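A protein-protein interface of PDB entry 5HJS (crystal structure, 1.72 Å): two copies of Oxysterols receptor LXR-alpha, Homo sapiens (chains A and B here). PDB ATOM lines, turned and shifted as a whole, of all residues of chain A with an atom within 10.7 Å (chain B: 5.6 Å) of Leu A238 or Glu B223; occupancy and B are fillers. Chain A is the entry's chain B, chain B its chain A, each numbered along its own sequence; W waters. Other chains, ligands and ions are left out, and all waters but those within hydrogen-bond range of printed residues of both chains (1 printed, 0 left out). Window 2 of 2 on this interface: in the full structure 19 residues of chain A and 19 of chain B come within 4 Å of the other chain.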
ATOM      1  N   LEU A 185      21.723  23.775  -6.733  1.00  0.00           N
ATOM      2  CA  LEU A 185      22.895  23.426  -7.550  1.00  0.00           C
ATOM      3  C   LEU A 185      23.966  22.712  -6.757  1.00  0.00           C
ATOM      4  O   LEU A 185      24.738  21.954  -7.347  1.00  0.00           O
ATOM      5  CB  LEU A 185      23.530  24.661  -8.242  1.00  0.00           C
ATOM      6  CG  LEU A 185      22.883  25.230  -9.487  1.00  0.00           C
ATOM      7  CD1 LEU A 185      23.661  26.410  -9.969  1.00  0.00           C
ATOM      8  CD2 LEU A 185      22.872  24.237 -10.609  1.00  0.00           C
ATOM      9  N   LEU A 187      26.885  23.815  -5.061  1.00  0.00           N
ATOM     10  CA  LEU A 187      28.215  24.125  -5.553  1.00  0.00           C
ATOM     11  C   LEU A 187      29.222  23.934  -4.471  1.00  0.00           C
ATOM     12  O   LEU A 187      28.927  24.171  -3.311  1.00  0.00           O
ATOM     13  CB  LEU A 187      28.304  25.562  -6.091  1.00  0.00           C
ATOM     14  CG  LEU A 187      27.362  25.951  -7.212  1.00  0.00           C
ATOM     15  CD1 LEU A 187      27.811  27.238  -7.818  1.00  0.00           C
ATOM     16  CD2 LEU A 187      27.264  24.871  -8.256  1.00  0.00           C
ATOM     17  N   GLU A 191      33.899  25.740  -7.210  1.00  0.00           N
ATOM     18  CA  GLU A 191      32.889  26.313  -8.097  1.00  0.00           C
ATOM     19  C   GLU A 191      32.471  27.696  -7.625  1.00  0.00           C
ATOM     20  O   GLU A 191      32.279  28.575  -8.455  1.00  0.00           O
ATOM     21  CB  GLU A 191      31.687  25.351  -8.207  1.00  0.00           C
ATOM     22  CG  GLU A 191      32.073  24.082  -8.950  1.00  0.00           C
ATOM     23  CD  GLU A 191      31.291  22.810  -8.683  1.00  0.00           C
ATOM     24  OE1 GLU A 191      30.522  22.757  -7.697  1.00  0.00           O
ATOM     25  OE2 GLU A 191      31.444  21.858  -9.481  1.00  0.00           O
ATOM     26  N   LEU A 225      36.600  26.498 -15.023  1.00  0.00           N
ATOM     27  CA  LEU A 225      35.346  26.021 -14.430  1.00  0.00           C
ATOM     28  C   LEU A 225      34.807  24.865 -15.260  1.00  0.00           C
ATOM     29  O   LEU A 225      34.407  23.848 -14.693  1.00  0.00           O
ATOM     30  CB  LEU A 225      34.274  27.132 -14.313  1.00  0.00           C
ATOM     31  CG  LEU A 225      32.895  26.761 -13.683  1.00  0.00           C
ATOM     32  CD1 LEU A 225      33.007  26.482 -12.185  1.00  0.00           C
ATOM     33  CD2 LEU A 225      31.900  27.895 -13.876  1.00  0.00           C
ATOM     34  N   HIS A 226      34.827  24.994 -16.593  1.00  0.00           N
ATOM     35  CA  HIS A 226      34.321  23.932 -17.475  1.00  0.00           C
ATOM     36  C   HIS A 226      35.041  22.599 -17.220  1.00  0.00           C
ATOM     37  O   HIS A 226      34.401  21.574 -17.021  1.00  0.00           O
ATOM     38  CB  HIS A 226      34.482  24.353 -18.942  1.00  0.00           C
ATOM     39  CG  HIS A 226      33.716  23.508 -19.916  1.00  0.00           C
ATOM     40  ND1 HIS A 226      33.660  23.837 -21.259  1.00  0.00           N
ATOM     41  CD2 HIS A 226      32.995  22.379 -19.715  1.00  0.00           C
ATOM     42  CE1 HIS A 226      32.932  22.890 -21.829  1.00  0.00           C
ATOM     43  NE2 HIS A 226      32.495  22.004 -20.930  1.00  0.00           N
ATOM     44  N   VAL A 229      34.298  21.276 -13.591  1.00  0.00           N
ATOM     45  CA  VAL A 229      32.936  20.742 -13.526  1.00  0.00           C
ATOM     46  C   VAL A 229      32.810  19.383 -14.231  1.00  0.00           C
ATOM     47  O   VAL A 229      32.007  18.563 -13.800  1.00  0.00           O
ATOM     48  CB  VAL A 229      31.883  21.773 -14.014  1.00  0.00           C
ATOM     49  CG1 VAL A 229      30.486  21.161 -14.061  1.00  0.00           C
ATOM     50  CG2 VAL A 229      31.897  22.998 -13.109  1.00  0.00           C
ATOM     51  N   SER A 230      33.597  19.145 -15.296  1.00  0.00           N
ATOM     52  CA  SER A 230      33.611  17.869 -16.028  1.00  0.00           C
ATOM     53  C   SER A 230      34.172  16.700 -15.164  1.00  0.00           C
ATOM     54  O   SER A 230      33.915  15.535 -15.462  1.00  0.00           O
ATOM     55  CB  SER A 230      34.432  18.020 -17.302  1.00  0.00           C
ATOM     56  OG  SER A 230      33.802  18.975 -18.140  1.00  0.00           O
ATOM     57  N   HIS A 232      33.819  16.966 -11.510  1.00  0.00           N
ATOM     58  CA  HIS A 232      32.863  16.942 -10.412  1.00  0.00           C
ATOM     59  C   HIS A 232      31.534  16.341 -10.813  1.00  0.00           C
ATOM     60  O   HIS A 232      30.936  15.618 -10.012  1.00  0.00           O
ATOM     61  CB  HIS A 232      32.694  18.351  -9.784  1.00  0.00           C
ATOM     62  CG  HIS A 232      31.866  18.408  -8.533  1.00  0.00           C
ATOM     63  ND1 HIS A 232      31.231  19.572  -8.151  1.00  0.00           N
ATOM     64  CD2 HIS A 232      31.618  17.461  -7.600  1.00  0.00           C
ATOM     65  CE1 HIS A 232      30.617  19.304  -7.007  1.00  0.00           C
ATOM     66  NE2 HIS A 232      30.820  18.047  -6.634  1.00  0.00           N
ATOM     67  N   HIS A 233      31.073  16.627 -12.039  1.00  0.00           N
ATOM     68  CA  HIS A 233      29.798  16.119 -12.557  1.00  0.00           C
ATOM     69  C   HIS A 233      30.070  15.477 -13.912  1.00  0.00           C
ATOM     70  O   HIS A 233      29.700  16.051 -14.939  1.00  0.00           O
ATOM     71  CB  HIS A 233      28.805  17.273 -12.685  1.00  0.00           C
ATOM     72  CG  HIS A 233      28.457  17.880 -11.365  1.00  0.00           C
ATOM     73  ND1 HIS A 233      27.624  17.241 -10.486  1.00  0.00           N
ATOM     74  CD2 HIS A 233      28.846  19.057 -10.824  1.00  0.00           C
ATOM     75  CE1 HIS A 233      27.532  18.029  -9.434  1.00  0.00           C
ATOM     76  NE2 HIS A 233      28.236  19.143  -9.603  1.00  0.00           N
ATOM     77  N   PRO A 234      30.757  14.310 -13.951  1.00  0.00           N
ATOM     78  CA  PRO A 234      31.091  13.696 -15.248  1.00  0.00           C
ATOM     79  C   PRO A 234      29.925  13.168 -16.085  1.00  0.00           C
ATOM     80  O   PRO A 234      30.118  12.925 -17.267  1.00  0.00           O
ATOM     81  CB  PRO A 234      32.042  12.552 -14.850  1.00  0.00           C
ATOM     82  CG  PRO A 234      31.565  12.142 -13.511  1.00  0.00           C
ATOM     83  CD  PRO A 234      31.258  13.471 -12.840  1.00  0.00           C
ATOM     84  N   HIS A 235      28.744  12.988 -15.495  1.00  0.00           N
ATOM     85  CA  HIS A 235      27.598  12.479 -16.249  1.00  0.00           C
ATOM     86  C   HIS A 235      26.493  13.520 -16.429  1.00  0.00           C
ATOM     87  O   HIS A 235      25.401  13.162 -16.853  1.00  0.00           O
ATOM     88  CB  HIS A 235      27.067  11.161 -15.638  1.00  0.00           C
ATOM     89  CG  HIS A 235      28.136  10.123 -15.456  1.00  0.00           C
ATOM     90  ND1 HIS A 235      28.838   9.602 -16.540  1.00  0.00           N
ATOM     91  CD2 HIS A 235      28.612   9.564 -14.318  1.00  0.00           C
ATOM     92  CE1 HIS A 235      29.703   8.742 -16.029  1.00  0.00           C
ATOM     93  NE2 HIS A 235      29.602   8.679 -14.698  1.00  0.00           N
ATOM     94  N   ASP A 236      26.787  14.815 -16.143  1.00  0.00           N
ATOM     95  CA  ASP A 236      25.811  15.893 -16.296  1.00  0.00           C
ATOM     96  C   ASP A 236      26.443  17.120 -16.946  1.00  0.00           C
ATOM     97  O   ASP A 236      26.967  18.000 -16.258  1.00  0.00           O
ATOM     98  CB  ASP A 236      25.113  16.216 -14.961  1.00  0.00           C
ATOM     99  CG  ASP A 236      23.936  17.178 -15.082  1.00  0.00           C
ATOM    100  OD1 ASP A 236      23.625  17.593 -16.210  1.00  0.00           O
ATOM    101  OD2 ASP A 236      23.345  17.517 -14.051  1.00  0.00           O
ATOM    102  N   ARG A 237      26.391  17.171 -18.283  1.00  0.00           N
ATOM    103  CA  ARG A 237      26.947  18.268 -19.093  1.00  0.00           C
ATOM    104  C   ARG A 237      26.195  19.612 -18.931  1.00  0.00           C
ATOM    105  O   ARG A 237      26.663  20.616 -19.456  1.00  0.00           O
ATOM    106  CB  ARG A 237      27.008  17.882 -20.586  1.00  0.00           C
ATOM    107  CG  ARG A 237      28.009  16.793 -20.943  1.00  0.00           C
ATOM    108  CD  ARG A 237      27.818  16.349 -22.383  1.00  0.00           C
ATOM    109  NE  ARG A 237      29.042  16.487 -23.182  1.00  0.00           N
ATOM    110  CZ  ARG A 237      29.926  15.511 -23.392  1.00  0.00           C
ATOM    111  NH1 ARG A 237      31.004  15.734 -24.134  1.00  0.00           N
ATOM    112  NH2 ARG A 237      29.739  14.308 -22.863  1.00  0.00           N
ATOM    113  N   LEU A 238      25.038  19.625 -18.231  1.00  0.00           N
ATOM    114  CA  LEU A 238      24.243  20.823 -17.989  1.00  0.00           C
ATOM    115  C   LEU A 238      24.714  21.578 -16.751  1.00  0.00           C
ATOM    116  O   LEU A 238      24.394  22.745 -16.627  1.00  0.00           O
ATOM    117  CB  LEU A 238      22.750  20.505 -17.857  1.00  0.00           C
ATOM    118  CG  LEU A 238      21.950  20.550 -19.172  1.00  0.00           C
ATOM    119  CD1 LEU A 238      20.607  19.893 -19.008  1.00  0.00           C
ATOM    120  CD2 LEU A 238      21.813  21.972 -19.706  1.00  0.00           C
ATOM    121  N   MET A 239      25.486  20.936 -15.847  1.00  0.00           N
ATOM    122  CA  MET A 239      25.969  21.595 -14.634  1.00  0.00           C
ATOM    123  C   MET A 239      26.815  22.835 -14.930  1.00  0.00           C
ATOM    124  O   MET A 239      26.621  23.841 -14.274  1.00  0.00           O
ATOM    125  CB  MET A 239      26.678  20.620 -13.702  1.00  0.00           C
ATOM    126  CG  MET A 239      25.715  19.706 -12.942  1.00  0.00           C
ATOM    127  SD  MET A 239      24.362  20.512 -12.055  1.00  0.00           S
ATOM    128  CE  MET A 239      25.180  21.205 -10.669  1.00  0.00           C
ATOM    129  N   PHE A 240      27.716  22.785 -15.938  1.00  0.00           N
ATOM    130  CA  PHE A 240      28.541  23.949 -16.330  1.00  0.00           C
ATOM    131  C   PHE A 240      27.686  25.152 -16.814  1.00  0.00           C
ATOM    132  O   PHE A 240      27.781  26.214 -16.173  1.00  0.00           O
ATOM    133  CB  PHE A 240      29.607  23.554 -17.370  1.00  0.00           C
ATOM    134  CG  PHE A 240      30.343  24.689 -18.047  1.00  0.00           C
ATOM    135  CD1 PHE A 240      31.128  25.576 -17.305  1.00  0.00           C
ATOM    136  CD2 PHE A 240      30.283  24.851 -19.430  1.00  0.00           C
ATOM    137  CE1 PHE A 240      31.828  26.623 -17.931  1.00  0.00           C
ATOM    138  CE2 PHE A 240      30.971  25.906 -20.064  1.00  0.00           C
ATOM    139  CZ  PHE A 240      31.736  26.790 -19.306  1.00  0.00           C
ATOM    140  N   PRO A 241      26.827  25.047 -17.875  1.00  0.00           N
ATOM    141  CA  PRO A 241      26.022  26.227 -18.259  1.00  0.00           C
ATOM    142  C   PRO A 241      25.055  26.672 -17.161  1.00  0.00           C
ATOM    143  O   PRO A 241      24.843  27.875 -17.036  1.00  0.00           O
ATOM    144  CB  PRO A 241      25.310  25.782 -19.540  1.00  0.00           C
ATOM    145  CG  PRO A 241      25.309  24.294 -19.476  1.00  0.00           C
ATOM    146  CD  PRO A 241      26.585  23.920 -18.804  1.00  0.00           C
ATOM    147  N   ARG A 242      24.516  25.741 -16.312  1.00  0.00           N
ATOM    148  CA  ARG A 242      23.618  26.111 -15.204  1.00  0.00           C
ATOM    149  C   ARG A 242      24.306  27.072 -14.227  1.00  0.00           C
ATOM    150  O   ARG A 242      23.680  28.028 -13.772  1.00  0.00           O
ATOM    151  CB  ARG A 242      23.087  24.868 -14.434  1.00  0.00           C
ATOM    152  CG  ARG A 242      22.012  24.101 -15.181  1.00  0.00           C
ATOM    153  CD  ARG A 242      21.567  22.870 -14.429  1.00  0.00           C
ATOM    154  NE  ARG A 242      20.760  23.221 -13.253  1.00  0.00           N
ATOM    155  CZ  ARG A 242      20.360  22.358 -12.327  1.00  0.00           C
ATOM    156  NH1 ARG A 242      20.681  21.079 -12.424  1.00  0.00           N
ATOM    157  NH2 ARG A 242      19.637  22.770 -11.294  1.00  0.00           N
ATOM    158  N   MET A 243      25.598  26.844 -13.924  1.00  0.00           N
ATOM    159  CA  MET A 243      26.335  27.731 -13.029  1.00  0.00           C
ATOM    160  C   MET A 243      26.549  29.072 -13.688  1.00  0.00           C
ATOM    161  O   MET A 243      26.416  30.087 -13.021  1.00  0.00           O
ATOM    162  CB  MET A 243      27.718  27.150 -12.629  1.00  0.00           C
ATOM    163  CG  MET A 243      27.644  25.895 -11.841  1.00  0.00           C
ATOM    164  SD  MET A 243      29.292  25.183 -11.610  1.00  0.00           S
ATOM    165  CE  MET A 243      28.803  23.466 -11.154  1.00  0.00           C
ATOM    166  N   LEU A 244      26.905  29.092 -14.991  1.00  0.00           N
ATOM    167  CA  LEU A 244      27.096  30.361 -15.687  1.00  0.00           C
ATOM    168  C   LEU A 244      25.821  31.147 -15.731  1.00  0.00           C
ATOM    169  O   LEU A 244      25.864  32.352 -15.561  1.00  0.00           O
ATOM    170  CB  LEU A 244      27.593  30.184 -17.126  1.00  0.00           C
ATOM    171  CG  LEU A 244      28.973  29.588 -17.354  1.00  0.00           C
ATOM    172  CD1 LEU A 244      29.221  29.491 -18.830  1.00  0.00           C
ATOM    173  CD2 LEU A 244      30.059  30.451 -16.728  1.00  0.00           C
ATOM    174  N   MET A 245      24.677  30.467 -15.956  1.00  0.00           N
ATOM    175  CA  MET A 245      23.358  31.098 -16.041  1.00  0.00           C
ATOM    176  C   MET A 245      22.968  31.777 -14.734  1.00  0.00           C
ATOM    177  O   MET A 245      22.111  32.652 -14.745  1.00  0.00           O
ATOM    178  CB  MET A 245      22.280  30.118 -16.513  1.00  0.00           C
ATOM    179  CG  MET A 245      22.439  29.652 -18.000  1.00  0.00           C
ATOM    180  SD  MET A 245      22.433  30.978 -19.242  1.00  0.00           S
ATOM    181  CE  MET A 245      20.678  31.343 -19.303  1.00  0.00           C
ATOM    182  N   LYS A 246      23.623  31.411 -13.610  1.00  0.00           N
ATOM    183  CA  LYS A 246      23.317  32.053 -12.345  1.00  0.00           C
ATOM    184  C   LYS A 246      23.840  33.478 -12.357  1.00  0.00           C
ATOM    185  O   LYS A 246      23.293  34.306 -11.656  1.00  0.00           O
ATOM    186  CB  LYS A 246      23.780  31.229 -11.130  1.00  0.00           C
ATOM    187  CG  LYS A 246      22.902  29.984 -10.924  1.00  0.00           C
ATOM    188  CD  LYS A 246      21.620  30.328 -10.147  1.00  0.00           C
ATOM    189  CE  LYS A 246      20.619  29.206 -10.073  1.00  0.00           C
ATOM    190  NZ  LYS A 246      19.772  29.153 -11.282  1.00  0.00           N
ATOM    191  N   GLN B  46      17.512  17.272 -31.882  1.00  0.00           N
ATOM    192  CA  GLN B  46      18.012  18.641 -31.714  1.00  0.00           C
ATOM    193  C   GLN B  46      18.175  19.312 -33.091  1.00  0.00           C
ATOM    194  O   GLN B  46      17.791  20.460 -33.250  1.00  0.00           O
ATOM    195  CB  GLN B  46      19.347  18.627 -30.969  1.00  0.00           C
ATOM    196  CG  GLN B  46      19.239  18.136 -29.524  1.00  0.00           C
ATOM    197  CD  GLN B  46      20.606  17.957 -28.924  1.00  0.00           C
ATOM    198  OE1 GLN B  46      21.541  17.508 -29.576  1.00  0.00           O
ATOM    199  NE2 GLN B  46      20.762  18.305 -27.667  1.00  0.00           N
ATOM    200  N   GLN B 218      14.413  25.523 -20.887  1.00  0.00           N
ATOM    201  CA  GLN B 218      15.615  26.294 -21.150  1.00  0.00           C
ATOM    202  C   GLN B 218      16.820  25.367 -21.313  1.00  0.00           C
ATOM    203  O   GLN B 218      17.651  25.622 -22.183  1.00  0.00           O
ATOM    204  CB  GLN B 218      15.914  27.233 -20.003  1.00  0.00           C
ATOM    205  CG  GLN B 218      16.888  28.322 -20.407  1.00  0.00           C
ATOM    206  CD  GLN B 218      17.295  29.172 -19.247  1.00  0.00           C
ATOM    207  OE1 GLN B 218      17.617  28.683 -18.172  1.00  0.00           O
ATOM    208  NE2 GLN B 218      17.310  30.456 -19.445  1.00  0.00           N
ATOM    209  N   HIS B 219      16.914  24.305 -20.479  1.00  0.00           N
ATOM    210  CA  HIS B 219      18.020  23.338 -20.543  1.00  0.00           C
ATOM    211  C   HIS B 219      18.042  22.566 -21.851  1.00  0.00           C
ATOM    212  O   HIS B 219      19.135  22.246 -22.315  1.00  0.00           O
ATOM    213  CB  HIS B 219      18.024  22.416 -19.314  1.00  0.00           C
ATOM    214  CG  HIS B 219      18.311  23.158 -18.038  1.00  0.00           C
ATOM    215  ND1 HIS B 219      18.074  22.580 -16.799  1.00  0.00           N
ATOM    216  CD2 HIS B 219      18.774  24.421 -17.850  1.00  0.00           C
ATOM    217  CE1 HIS B 219      18.414  23.493 -15.903  1.00  0.00           C
ATOM    218  NE2 HIS B 219      18.825  24.623 -16.485  1.00  0.00           N
ATOM    219  N   THR B 220      16.868  22.358 -22.510  1.00  0.00           N
ATOM    220  CA  THR B 220      16.854  21.664 -23.806  1.00  0.00           C
ATOM    221  C   THR B 220      17.448  22.549 -24.873  1.00  0.00           C
ATOM    222  O   THR B 220      18.166  22.042 -25.727  1.00  0.00           O
ATOM    223  CB  THR B 220      15.497  21.083 -24.179  1.00  0.00           C
ATOM    224  OG1 THR B 220      14.626  22.138 -24.564  1.00  0.00           O
ATOM    225  CG2 THR B 220      14.869  20.272 -23.043  1.00  0.00           C
ATOM    226  N   TYR B 221      17.214  23.869 -24.811  1.00  0.00           N
ATOM    227  CA  TYR B 221      17.798  24.817 -25.787  1.00  0.00           C
ATOM    228  C   TYR B 221      19.280  25.026 -25.519  1.00  0.00           C
ATOM    229  O   TYR B 221      20.064  25.151 -26.446  1.00  0.00           O
ATOM    230  CB  TYR B 221      17.021  26.165 -25.838  1.00  0.00           C
ATOM    231  CG  TYR B 221      15.590  25.939 -26.282  1.00  0.00           C
ATOM    232  CD1 TYR B 221      15.282  25.727 -27.619  1.00  0.00           C
ATOM    233  CD2 TYR B 221      14.563  25.831 -25.354  1.00  0.00           C
ATOM    234  CE1 TYR B 221      13.985  25.433 -28.024  1.00  0.00           C
ATOM    235  CE2 TYR B 221      13.261  25.530 -25.745  1.00  0.00           C
ATOM    236  CZ  TYR B 221      12.972  25.354 -27.088  1.00  0.00           C
ATOM    237  OH  TYR B 221      11.690  25.076 -27.490  1.00  0.00           O
ATOM    238  N   VAL B 222      19.667  25.070 -24.246  1.00  0.00           N
ATOM    239  CA  VAL B 222      21.069  25.253 -23.853  1.00  0.00           C
ATOM    240  C   VAL B 222      21.910  24.048 -24.390  1.00  0.00           C
ATOM    241  O   VAL B 222      23.005  24.242 -24.958  1.00  0.00           O
ATOM    242  CB  VAL B 222      21.214  25.446 -22.299  1.00  0.00           C
ATOM    243  CG1 VAL B 222      22.664  25.238 -21.857  1.00  0.00           C
ATOM    244  CG2 VAL B 222      20.696  26.822 -21.849  1.00  0.00           C
ATOM    245  N   GLU B 223      21.369  22.820 -24.229  1.00  0.00           N
ATOM    246  CA  GLU B 223      22.009  21.581 -24.667  1.00  0.00           C
ATOM    247  C   GLU B 223      22.108  21.570 -26.181  1.00  0.00           C
ATOM    248  O   GLU B 223      23.146  21.175 -26.727  1.00  0.00           O
ATOM    249  CB  GLU B 223      21.199  20.351 -24.224  1.00  0.00           C
ATOM    250  CG  GLU B 223      21.547  19.821 -22.847  1.00  0.00           C
ATOM    251  CD  GLU B 223      21.358  18.324 -22.702  1.00  0.00           C
ATOM    252  OE1 GLU B 223      20.198  17.855 -22.779  1.00  0.00           O
ATOM    253  OE2 GLU B 223      22.374  17.618 -22.514  1.00  0.00           O
ATOM    254  N   ALA B 224      21.025  22.003 -26.865  1.00  0.00           N
ATOM    255  CA  ALA B 224      21.021  22.066 -28.335  1.00  0.00           C
ATOM    256  C   ALA B 224      22.038  23.066 -28.866  1.00  0.00           C
ATOM    257  O   ALA B 224      22.704  22.778 -29.863  1.00  0.00           O
ATOM    258  CB  ALA B 224      19.627  22.375 -28.843  1.00  0.00           C
ATOM    259  N   LEU B 225      22.183  24.223 -28.177  1.00  0.00           N
ATOM    260  CA  LEU B 225      23.155  25.257 -28.524  1.00  0.00           C
ATOM    261  C   LEU B 225      24.566  24.690 -28.348  1.00  0.00           C
ATOM    262  O   LEU B 225      25.391  24.844 -29.242  1.00  0.00           O
ATOM    263  CB  LEU B 225      22.977  26.506 -27.658  1.00  0.00           C
ATOM    264  CG  LEU B 225      23.898  27.694 -27.976  1.00  0.00           C
ATOM    265  CD1 LEU B 225      23.595  28.304 -29.381  1.00  0.00           C
ATOM    266  CD2 LEU B 225      23.804  28.783 -26.904  1.00  0.00           C
ATOM    267  N   HIS B 226      24.827  24.007 -27.222  1.00  0.00           N
ATOM    268  CA  HIS B 226      26.133  23.416 -26.945  1.00  0.00           C
ATOM    269  C   HIS B 226      26.538  22.443 -28.048  1.00  0.00           C
ATOM    270  O   HIS B 226      27.637  22.543 -28.590  1.00  0.00           O
ATOM    271  CB  HIS B 226      26.122  22.688 -25.590  1.00  0.00           C
ATOM    272  CG  HIS B 226      27.496  22.398 -25.048  1.00  0.00           C
ATOM    273  ND1 HIS B 226      27.673  21.857 -23.773  1.00  0.00           N
ATOM    274  CD2 HIS B 226      28.715  22.629 -25.591  1.00  0.00           C
ATOM    275  CE1 HIS B 226      28.983  21.751 -23.599  1.00  0.00           C
ATOM    276  NE2 HIS B 226      29.654  22.204 -24.667  1.00  0.00           N
ATOM    277  N   ALA B 227      25.637  21.517 -28.385  1.00  0.00           N
ATOM    278  CA  ALA B 227      25.874  20.504 -29.402  1.00  0.00           C
ATOM    279  C   ALA B 227      26.031  21.149 -30.768  1.00  0.00           C
ATOM    280  O   ALA B 227      26.942  20.779 -31.509  1.00  0.00           O
ATOM    281  CB  ALA B 227      24.745  19.516 -29.390  1.00  0.00           C
ATOM    282  N   TYR B 228      25.221  22.176 -31.073  1.00  0.00           N
ATOM    283  CA  TYR B 228      25.331  22.895 -32.352  1.00  0.00           C
ATOM    284  C   TYR B 228      26.663  23.639 -32.482  1.00  0.00           C
ATOM    285  O   TYR B 228      27.359  23.503 -33.495  1.00  0.00           O
ATOM    286  CB  TYR B 228      24.160  23.871 -32.539  1.00  0.00           C
ATOM    287  CG  TYR B 228      24.216  24.579 -33.872  1.00  0.00           C
ATOM    288  CD1 TYR B 228      23.665  24.002 -35.017  1.00  0.00           C
ATOM    289  CD2 TYR B 228      24.815  25.827 -33.993  1.00  0.00           C
ATOM    290  CE1 TYR B 228      23.711  24.665 -36.249  1.00  0.00           C
ATOM    291  CE2 TYR B 228      24.890  26.481 -35.216  1.00  0.00           C
ATOM    292  CZ  TYR B 228      24.342  25.894 -36.341  1.00  0.00           C
ATOM    293  OH  TYR B 228      24.407  26.585 -37.524  1.00  0.00           O
HETATM  294  O   HOH W   1      25.731  21.357 -21.889  1.00  0.00           O
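The side-chain sulfur of Met A239 is in hydrogen-bond range of the guanidinium group of Arg A242, at 3.7 Å. The side-chain carboxylate of Asp A236 sits close to the backbone NH of Leu A238 (3.2 Å).
Among the printed residues, merely in contact across the chains: Arg A242 with His B219 (3.5 Å), Met A245 with Gln B218 (3.5 Å), Pro A241 with Val B222 (3.6 Å), Leu A238 with His B219 (3.6 Å) and Leu A238 with Glu B223 (3.8 Å).
Leu A185 touches none of the printed residues of chain B. Printed residues of chain B within 4 Å of Leu A238: His B219 (3.6 Å) and Glu B223 (3.8 Å). Of the printed residues of chain B, Pro A241 touches Val B222 (3.6 Å). Printed residues of chain B within 4 Å of Arg A242: His B219. Met A243 touches none of the printed residues of chain B. Of the printed residues of chain B, Met A245 touches Gln B218 (3.5 Å). Printed residues of chain A within 4 Å of Gln B218: Met A245. His B219 touches two residues of chain A. Printed residues of chain A within 4 Å of Val B222: Pro A241. Ala B224 touches none of the printed residues of chain A. The nearest printed residue of chain B that does not touch Leu A238 is Val B222 (4.002 Å).
Along chain B the printed residues that touch a printed residue of chain A span positions 218 to 223. Of the 22 printed residues of chain A, 4 touch a printed residue of chain B. Hydrophobic or aromatic side chains of chain A within 4 Å of the printed part of chain B: Leu A238, Pro A241 and Met A245. Among the printed residues, 5 pairs touch across the chains. Among the printed residues, no Asp or Glu carboxylate lies within 4 Å of a Lys or Arg side-chain nitrogen of the other chain.
Positions printed for both chains: 225 and 226.
Water W1 lies within hydrogen-bond range of O of Arg A237 (2.7 Å) and ND1 of His B226 (2.8 Å).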
